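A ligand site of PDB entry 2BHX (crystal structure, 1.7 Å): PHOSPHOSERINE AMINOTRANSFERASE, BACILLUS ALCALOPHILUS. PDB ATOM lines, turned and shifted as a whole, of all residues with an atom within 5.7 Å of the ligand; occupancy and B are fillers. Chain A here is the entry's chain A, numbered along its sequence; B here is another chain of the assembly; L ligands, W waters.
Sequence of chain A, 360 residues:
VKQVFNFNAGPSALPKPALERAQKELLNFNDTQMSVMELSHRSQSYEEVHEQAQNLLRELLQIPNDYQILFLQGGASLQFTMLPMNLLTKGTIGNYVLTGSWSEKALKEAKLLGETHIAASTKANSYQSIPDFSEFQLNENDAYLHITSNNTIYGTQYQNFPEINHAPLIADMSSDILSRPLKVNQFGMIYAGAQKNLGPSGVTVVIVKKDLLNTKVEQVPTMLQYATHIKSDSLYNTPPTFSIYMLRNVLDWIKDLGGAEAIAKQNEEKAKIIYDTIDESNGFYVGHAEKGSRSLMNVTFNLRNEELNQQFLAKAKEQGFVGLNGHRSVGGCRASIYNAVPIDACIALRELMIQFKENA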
ATOM      1  N   GLY A  74      31.814  17.924 -29.363  1.00  0.00           N
ATOM      2  CA  GLY A  74      30.493  18.534 -29.299  1.00  0.00           C
ATOM      3  C   GLY A  74      30.063  18.892 -27.889  1.00  0.00           C
ATOM      4  O   GLY A  74      29.064  19.593 -27.692  1.00  0.00           O
ATOM      5  N   GLY A  75      30.823  18.405 -26.915  1.00  0.00           N
ATOM      6  CA  GLY A  75      30.489  18.764 -25.536  1.00  0.00           C
ATOM      7  C   GLY A  75      29.324  17.935 -25.007  1.00  0.00           C
ATOM      8  O   GLY A  75      28.668  17.148 -25.703  1.00  0.00           O
ATOM      9  N   ALA A  76      29.067  18.130 -23.706  1.00  0.00           N
ATOM     10  CA  ALA A  76      27.914  17.427 -23.120  1.00  0.00           C
ATOM     11  C   ALA A  76      26.654  17.904 -23.796  1.00  0.00           C
ATOM     12  O   ALA A  76      25.654  17.194 -23.955  1.00  0.00           O
ATOM     13  CB  ALA A  76      27.898  17.688 -21.614  1.00  0.00           C
ATOM     14  N   SER A  77      26.707  19.170 -24.192  1.00  0.00           N
ATOM     15  CA  SER A  77      25.514  19.757 -24.816  1.00  0.00           C
ATOM     16  C   SER A  77      25.103  18.984 -26.037  1.00  0.00           C
ATOM     17  O   SER A  77      23.900  18.802 -26.243  1.00  0.00           O
ATOM     18  CB  SER A  77      25.718  21.225 -25.173  1.00  0.00           C
ATOM     19  OG  SER A  77      25.856  21.978 -23.973  1.00  0.00           O
ATOM     20  N   LEU A  78      26.051  18.518 -26.848  1.00  0.00           N
ATOM     21  CA  LEU A  78      25.643  17.737 -28.007  1.00  0.00           C
ATOM     22  C   LEU A  78      25.037  16.402 -27.564  1.00  0.00           C
ATOM     23  O   LEU A  78      24.150  15.876 -28.246  1.00  0.00           O
ATOM     24  CB  LEU A  78      26.805  17.454 -28.977  1.00  0.00           C
ATOM     25  CG  LEU A  78      26.374  16.773 -30.282  1.00  0.00           C
ATOM     26  CD1 LEU A  78      25.350  17.628 -31.008  1.00  0.00           C
ATOM     27  CD2 LEU A  78      27.572  16.473 -31.171  1.00  0.00           C
ATOM     28  N   PHE A  80      23.073  16.042 -25.120  1.00  0.00           N
ATOM     29  CA  PHE A  80      21.663  16.279 -24.791  1.00  0.00           C
ATOM     30  C   PHE A  80      20.738  15.951 -25.959  1.00  0.00           C
ATOM     31  O   PHE A  80      19.609  15.488 -25.774  1.00  0.00           O
ATOM     32  CB  PHE A  80      21.441  17.743 -24.405  1.00  0.00           C
ATOM     33  CG  PHE A  80      22.106  18.234 -23.134  1.00  0.00           C
ATOM     34  CD1 PHE A  80      22.236  19.605 -22.924  1.00  0.00           C
ATOM     35  CD2 PHE A  80      22.582  17.331 -22.178  1.00  0.00           C
ATOM     36  CE1 PHE A  80      22.831  20.102 -21.761  1.00  0.00           C
ATOM     37  CE2 PHE A  80      23.149  17.829 -21.030  1.00  0.00           C
ATOM     38  CZ  PHE A  80      23.278  19.190 -20.810  1.00  0.00           C
ATOM     39  N   TRP A 102      21.364  22.286 -15.649  1.00  0.00           N
ATOM     40  CA  TRP A 102      21.819  21.329 -16.665  1.00  0.00           C
ATOM     41  C   TRP A 102      20.787  20.230 -16.888  1.00  0.00           C
ATOM     42  O   TRP A 102      20.588  19.776 -18.021  1.00  0.00           O
ATOM     43  CB  TRP A 102      23.189  20.716 -16.347  1.00  0.00           C
ATOM     44  CG  TRP A 102      24.252  21.763 -16.463  1.00  0.00           C
ATOM     45  CD1 TRP A 102      25.052  22.263 -15.472  1.00  0.00           C
ATOM     46  CD2 TRP A 102      24.632  22.458 -17.654  1.00  0.00           C
ATOM     47  NE1 TRP A 102      25.908  23.216 -15.966  1.00  0.00           N
ATOM     48  CE2 TRP A 102      25.672  23.345 -17.309  1.00  0.00           C
ATOM     49  CE3 TRP A 102      24.197  22.390 -18.982  1.00  0.00           C
ATOM     50  CZ2 TRP A 102      26.290  24.181 -18.242  1.00  0.00           C
ATOM     51  CZ3 TRP A 102      24.817  23.221 -19.898  1.00  0.00           C
ATOM     52  CH2 TRP A 102      25.837  24.111 -19.544  1.00  0.00           C
ATOM     53  N   THR A 148      21.265  13.976 -13.640  1.00  0.00           N
ATOM     54  CA  THR A 148      22.468  14.809 -13.611  1.00  0.00           C
ATOM     55  C   THR A 148      23.162  14.542 -12.277  1.00  0.00           C
ATOM     56  O   THR A 148      22.704  14.993 -11.225  1.00  0.00           O
ATOM     57  CB  THR A 148      22.110  16.285 -13.795  1.00  0.00           C
ATOM     58  OG1 THR A 148      21.210  16.382 -14.926  1.00  0.00           O
ATOM     59  CG2 THR A 148      23.344  17.118 -14.105  1.00  0.00           C
ATOM     60  N   ASN A 150      25.944  15.468 -10.744  1.00  0.00           N
ATOM     61  CA  ASN A 150      26.407  16.667 -10.045  1.00  0.00           C
ATOM     62  C   ASN A 150      25.865  17.916 -10.737  1.00  0.00           C
ATOM     63  O   ASN A 150      26.094  18.152 -11.932  1.00  0.00           O
ATOM     64  CB  ASN A 150      27.942  16.709  -9.977  1.00  0.00           C
ATOM     65  CG  ASN A 150      28.452  17.835  -9.110  1.00  0.00           C
ATOM     66  OD1 ASN A 150      28.851  18.904  -9.587  1.00  0.00           O
ATOM     67  ND2 ASN A 150      28.444  17.649  -7.801  1.00  0.00           N
ATOM     68  N   ASN A 151      25.111  18.695  -9.968  1.00  0.00           N
ATOM     69  CA  ASN A 151      24.405  19.861 -10.502  1.00  0.00           C
ATOM     70  C   ASN A 151      25.291  21.082 -10.356  1.00  0.00           C
ATOM     71  O   ASN A 151      25.273  21.759  -9.345  1.00  0.00           O
ATOM     72  CB  ASN A 151      23.050  19.989  -9.776  1.00  0.00           C
ATOM     73  CG  ASN A 151      22.300  18.688  -9.905  1.00  0.00           C
ATOM     74  OD1 ASN A 151      21.726  18.375 -10.948  1.00  0.00           O
ATOM     75  ND2 ASN A 151      22.282  17.884  -8.853  1.00  0.00           N
ATOM     76  N   THR A 152      26.084  21.279 -11.421  1.00  0.00           N
ATOM     77  CA  THR A 152      27.229  22.169 -11.376  1.00  0.00           C
ATOM     78  C   THR A 152      26.902  23.582 -10.910  1.00  0.00           C
ATOM     79  O   THR A 152      27.695  24.252 -10.254  1.00  0.00           O
ATOM     80  CB  THR A 152      27.853  22.233 -12.791  1.00  0.00           C
ATOM     81  OG1 THR A 152      27.712  20.928 -13.331  1.00  0.00           O
ATOM     82  CG2 THR A 152      29.338  22.550 -12.699  1.00  0.00           C
ATOM     83  N   ASP A 172      24.307  12.491 -16.951  1.00  0.00           N
ATOM     84  CA  ASP A 172      25.243  13.578 -17.245  1.00  0.00           C
ATOM     85  C   ASP A 172      26.163  13.717 -16.025  1.00  0.00           C
ATOM     86  O   ASP A 172      25.782  14.318 -15.019  1.00  0.00           O
ATOM     87  CB  ASP A 172      24.507  14.871 -17.536  1.00  0.00           C
ATOM     88  CG  ASP A 172      25.393  16.073 -17.754  1.00  0.00           C
ATOM     89  OD1 ASP A 172      26.638  15.926 -17.680  1.00  0.00           O
ATOM     90  OD2 ASP A 172      24.805  17.158 -18.012  1.00  0.00           O
ATOM     91  N   MET A 173      27.371  13.147 -16.172  1.00  0.00           N
ATOM     92  CA  MET A 173      28.330  13.237 -15.065  1.00  0.00           C
ATOM     93  C   MET A 173      29.449  14.226 -15.340  1.00  0.00           C
ATOM     94  O   MET A 173      30.522  14.051 -14.771  1.00  0.00           O
ATOM     95  CB  MET A 173      28.909  11.849 -14.799  1.00  0.00           C
ATOM     96  CG  MET A 173      27.868  10.848 -14.298  1.00  0.00           C
ATOM     97  SD  MET A 173      28.698   9.394 -13.615  1.00  0.00           S
ATOM     98  CE  MET A 173      27.276   8.457 -13.012  1.00  0.00           C
ATOM     99  N   SER A 174      29.210  15.231 -16.178  1.00  0.00           N
ATOM    100  CA  SER A 174      30.247  16.194 -16.556  1.00  0.00           C
ATOM    101  C   SER A 174      31.082  16.696 -15.383  1.00  0.00           C
ATOM    102  O   SER A 174      32.309  16.726 -15.468  1.00  0.00           O
ATOM    103  CB  SER A 174      29.588  17.388 -17.245  1.00  0.00           C
ATOM    104  OG  SER A 174      28.997  16.999 -18.490  1.00  0.00           O
ATOM    105  N   SER A 175      30.415  17.082 -14.264  1.00  0.00           N
ATOM    106  CA  SER A 175      31.223  17.762 -13.230  1.00  0.00           C
ATOM    107  C   SER A 175      31.600  16.876 -12.054  1.00  0.00           C
ATOM    108  O   SER A 175      32.162  17.428 -11.096  1.00  0.00           O
ATOM    109  CB  SER A 175      30.502  19.043 -12.760  1.00  0.00           C
ATOM    110  OG  SER A 175      29.136  18.760 -12.471  1.00  0.00           O
ATOM    111  N   GLY A 193      31.467  16.136 -20.508  1.00  0.00           N
ATOM    112  CA  GLY A 193      32.501  16.924 -21.184  1.00  0.00           C
ATOM    113  C   GLY A 193      33.765  16.786 -20.339  1.00  0.00           C
ATOM    114  O   GLY A 193      33.754  16.800 -19.102  1.00  0.00           O
ATOM    115  N   GLN A 195      36.184  18.818 -19.717  1.00  0.00           N
ATOM    116  CA  GLN A 195      36.812  20.041 -19.226  1.00  0.00           C
ATOM    117  C   GLN A 195      36.470  20.360 -17.777  1.00  0.00           C
ATOM    118  O   GLN A 195      36.884  21.380 -17.227  1.00  0.00           O
ATOM    119  CB  GLN A 195      36.407  21.252 -20.070  1.00  0.00           C
ATOM    120  CG  GLN A 195      34.928  21.607 -19.950  1.00  0.00           C
ATOM    121  CD  GLN A 195      34.068  20.878 -20.952  1.00  0.00           C
ATOM    122  OE1 GLN A 195      34.442  19.840 -21.528  1.00  0.00           O
ATOM    123  NE2 GLN A 195      32.857  21.386 -21.173  1.00  0.00           N
ATOM    124  N   LYS A 196      35.667  19.494 -17.144  1.00  0.00           N
ATOM    125  CA  LYS A 196      35.423  19.885 -15.744  1.00  0.00           C
ATOM    126  C   LYS A 196      36.368  19.133 -14.840  1.00  0.00           C
ATOM    127  O   LYS A 196      37.095  19.642 -14.004  1.00  0.00           O
ATOM    128  CB  LYS A 196      33.966  19.663 -15.351  1.00  0.00           C
ATOM    129  CG  LYS A 196      32.928  20.256 -16.292  1.00  0.00           C
ATOM    130  CD  LYS A 196      32.396  21.548 -15.713  1.00  0.00           C
ATOM    131  CE  LYS A 196      31.691  22.399 -16.746  1.00  0.00           C
ATOM    132  NZ  LYS A 196      30.298  21.923 -16.959  1.00  0.00           N
ATOM    133  N   THR A 204      34.440  14.809 -25.304  1.00  0.00           N
ATOM    134  CA  THR A 204      33.384  14.380 -24.402  1.00  0.00           C
ATOM    135  C   THR A 204      33.493  12.873 -24.216  1.00  0.00           C
ATOM    136  O   THR A 204      33.522  12.168 -25.223  1.00  0.00           O
ATOM    137  CB  THR A 204      32.007  14.760 -24.996  1.00  0.00           C
ATOM    138  OG1 THR A 204      31.944  16.183 -25.035  1.00  0.00           O
ATOM    139  CG2 THR A 204      30.897  14.249 -24.106  1.00  0.00           C
ATOM    140  N   TYR A 338      37.122  20.627  -8.230  1.00  0.00           N
ATOM    141  CA  TYR A 338      37.341  19.377  -8.949  1.00  0.00           C
ATOM    142  C   TYR A 338      38.638  18.667  -8.530  1.00  0.00           C
ATOM    143  O   TYR A 338      39.422  19.273  -7.798  1.00  0.00           O
ATOM    144  CB  TYR A 338      37.426  19.685 -10.455  1.00  0.00           C
ATOM    145  CG  TYR A 338      36.189  20.376 -10.982  1.00  0.00           C
ATOM    146  CD1 TYR A 338      36.277  21.662 -11.504  1.00  0.00           C
ATOM    147  CD2 TYR A 338      34.951  19.747 -10.964  1.00  0.00           C
ATOM    148  CE1 TYR A 338      35.165  22.312 -11.997  1.00  0.00           C
ATOM    149  CE2 TYR A 338      33.826  20.403 -11.455  1.00  0.00           C
ATOM    150  CZ  TYR A 338      33.931  21.676 -11.976  1.00  0.00           C
ATOM    151  OH  TYR A 338      32.824  22.356 -12.470  1.00  0.00           O
ATOM    152  N   HIS B  41      35.882  29.555 -20.304  1.00  0.00           N
ATOM    153  CA  HIS B  41      35.601  30.120 -21.623  1.00  0.00           C
ATOM    154  C   HIS B  41      34.802  31.408 -21.505  1.00  0.00           C
ATOM    155  O   HIS B  41      34.563  32.103 -22.482  1.00  0.00           O
ATOM    156  CB  HIS B  41      34.863  29.106 -22.493  1.00  0.00           C
ATOM    157  CG  HIS B  41      33.543  28.683 -21.919  1.00  0.00           C
ATOM    158  ND1 HIS B  41      33.394  28.055 -20.708  1.00  0.00           N
ATOM    159  CD2 HIS B  41      32.295  28.809 -22.441  1.00  0.00           C
ATOM    160  CE1 HIS B  41      32.109  27.820 -20.495  1.00  0.00           C
ATOM    161  NE2 HIS B  41      31.420  28.272 -21.541  1.00  0.00           N
ATOM    162  N   GLN B  73      32.625  22.395 -33.029  1.00  0.00           N
ATOM    163  CA  GLN B  73      33.191  21.068 -32.897  1.00  0.00           C
ATOM    164  C   GLN B  73      32.538  20.122 -33.894  1.00  0.00           C
ATOM    165  O   GLN B  73      31.503  20.501 -34.474  1.00  0.00           O
ATOM    166  CB  GLN B  73      32.972  20.526 -31.470  1.00  0.00           C
ATOM    167  CG  GLN B  73      33.608  21.429 -30.397  1.00  0.00           C
ATOM    168  CD  GLN B  73      33.397  20.806 -29.021  1.00  0.00           C
ATOM    169  OE1 GLN B  73      33.916  19.708 -28.769  1.00  0.00           O
ATOM    170  NE2 GLN B  73      32.641  21.500 -28.176  1.00  0.00           N
ATOM    171  N   ASN B 237      28.025  26.801 -25.908  1.00  0.00           N
ATOM    172  CA  ASN B 237      28.551  25.839 -24.931  1.00  0.00           C
ATOM    173  C   ASN B 237      30.075  25.985 -24.903  1.00  0.00           C
ATOM    174  O   ASN B 237      30.615  26.933 -25.463  1.00  0.00           O
ATOM    175  CB  ASN B 237      28.143  24.395 -25.187  1.00  0.00           C
ATOM    176  CG  ASN B 237      28.805  23.741 -26.375  1.00  0.00           C
ATOM    177  OD1 ASN B 237      29.089  24.426 -27.382  1.00  0.00           O
ATOM    178  ND2 ASN B 237      29.036  22.455 -26.236  1.00  0.00           N
ATOM    179  N   THR B 238      30.739  25.088 -24.228  1.00  0.00           N
ATOM    180  CA  THR B 238      32.191  25.278 -24.048  1.00  0.00           C
ATOM    181  C   THR B 238      32.885  25.021 -25.386  1.00  0.00           C
ATOM    182  O   THR B 238      32.728  23.922 -25.935  1.00  0.00           O
ATOM    183  CB  THR B 238      32.723  24.327 -22.968  1.00  0.00           C
ATOM    184  OG1 THR B 238      31.956  24.424 -21.754  1.00  0.00           O
ATOM    185  CG2 THR B 238      34.170  24.694 -22.591  1.00  0.00           C
HETATM  186  N1  LIG L   1      26.283  19.327 -18.165  1.00  0.00           N
HETATM  187  C1  LIG L   1      26.899  19.587 -16.983  1.00  0.00           C
HETATM  188  C2  LIG L   1      26.425  18.957 -15.675  1.00  0.00           C
HETATM  189  C3  LIG L   1      27.916  20.498 -16.953  1.00  0.00           C
HETATM  190  O1  LIG L   1      28.475  20.774 -15.736  1.00  0.00           O
HETATM  191  C4  LIG L   1      28.279  21.142 -18.118  1.00  0.00           C
HETATM  192  C5  LIG L   1      29.589  21.975 -18.168  1.00  0.00           C
HETATM  193  C6  LIG L   1      27.612  20.903 -19.287  1.00  0.00           C
HETATM  194  C7  LIG L   1      26.609  19.973 -19.324  1.00  0.00           C
HETATM  195  C8  LIG L   1      27.998  21.642 -20.594  1.00  0.00           C
HETATM  196  O2  LIG L   1      29.066  20.966 -21.249  1.00  0.00           O
HETATM  197  P1  LIG L   1      29.567  21.515 -22.664  1.00  0.00           P
HETATM  198  O3  LIG L   1      29.847  22.943 -22.419  1.00  0.00           O
HETATM  199  O4  LIG L   1      28.405  21.273 -23.559  1.00  0.00           O
HETATM  200  O5  LIG L   1      30.741  20.685 -22.987  1.00  0.00           O
HETATM  201  O   HOH W   1      30.092  25.002 -18.306  1.00  0.00           O
HETATM  202  O   HOH W   2      28.243  25.082 -21.814  1.00  0.00           O
HETATM  203  O   HOH W   3      32.247  21.424 -25.120  1.00  0.00           O
HETATM  204  O   HOH W   4      30.567  18.921 -19.916  1.00  0.00           O
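Water W3 lies within hydrogen-bond range of the backbone carbonyl oxygen of Thr 238 of chain B (2.7 Å), an oxygen (O5) of the ligand (2.7 Å) and the side-chain amide nitrogen of Gln 73 of chain B (3.1 Å). Water W2 lies within hydrogen-bond range of O3 of the ligand and N of Thr 238 of chain B. Water W4 lies within hydrogen-bond range of OG of Ser 174 (2.9 Å), O2 of the ligand (2.9 Å) and N of Gly 193 (3.0 Å).
Gly 75 touches the ligand. Phe 80 touches the ligand (CZ to C7, 3.7 Å). Trp 102 touches the ligand. CG2 of Thr 148 touches C2 of the ligand, at 3.9 Å. Asn 150 touches the ligand. Ser 174 touches the ligand. Ser 175 touches the ligand (OG to O1, 3.9 Å). Hydrophobic or aromatic side chains within 4 Å of the ligand: Ala 76, Phe 80 and Trp 102. Of the 24 residues printed, 15 come within 4 Å of the ligand. Along chain A the residues within 4 Å of the ligand span positions 75 to 196.
The side-chain hydroxyl (OG) of Ser 175 is in hydrogen-bond range of the side-chain hydroxyl (OG1) of Thr 152 (2.7 Å). The side-chain carboxylate (OD1) of Asp 172 lies within hydrogen-bond range of the side-chain hydroxyl (OG) of Ser 174. The side-chain hydroxyl (OG1) of Thr 238 of chain B is in hydrogen-bond range of the side-chain amide nitrogen (NE2) of Gln 195 (3.2 Å). O of Thr 238 of chain B sits at hydrogen-bond distance from NE2 of Gln 73 of chain B (3.3 Å). ND2 of Asn 237 of chain B is in hydrogen-bond range of O of Gly 74 (3.2 Å). The backbone NH (N) of Gly 75 sits close to the side-chain hydroxyl (OG1) of Thr 204, at 3.1 Å. The side-chain hydroxyl (OG) of Ser 174 is in hydrogen-bond range of the backbone NH (N) of Gly 193 (3.3 Å). OG of Ser 175 sits at hydrogen-bond distance from OD1 of Asn 150.
The side-chain amino group of Lys 196 is covalently linked to a carbon (C5) of the ligand (1.4 Å). The side-chain hydroxyl of Thr 152 is in hydrogen-bond range of an oxygen (O1) of the ligand, at 2.5 Å. OD2 of Asp 172 is in hydrogen-bond range of N1 of the ligand, 2.6 Å away. An oxygen (O3) of the ligand lies within hydrogen-bond range of the backbone NH (N) of Thr 238 of chain B. OG1 of Thr 238 of chain B sits at hydrogen-bond distance from O3 of the ligand. O4 of the ligand sits at hydrogen-bond distance from N of Ser 77, at 2.8 Å. The side-chain hydroxyl (OG) of Ser 77 sits at hydrogen-bond distance from an oxygen (O4) of the ligand, at 2.7 Å. The side-chain amide nitrogen of Gln 195 is in hydrogen-bond range of an oxygen (O5) of the ligand (2.9 Å). An oxygen (O4) of the ligand sits at hydrogen-bond distance from the side-chain amide nitrogen (ND2) of Asn 237 of chain B. N of Ala 76 sits at hydrogen-bond distance from O5 of the ligand (3.1 Å).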
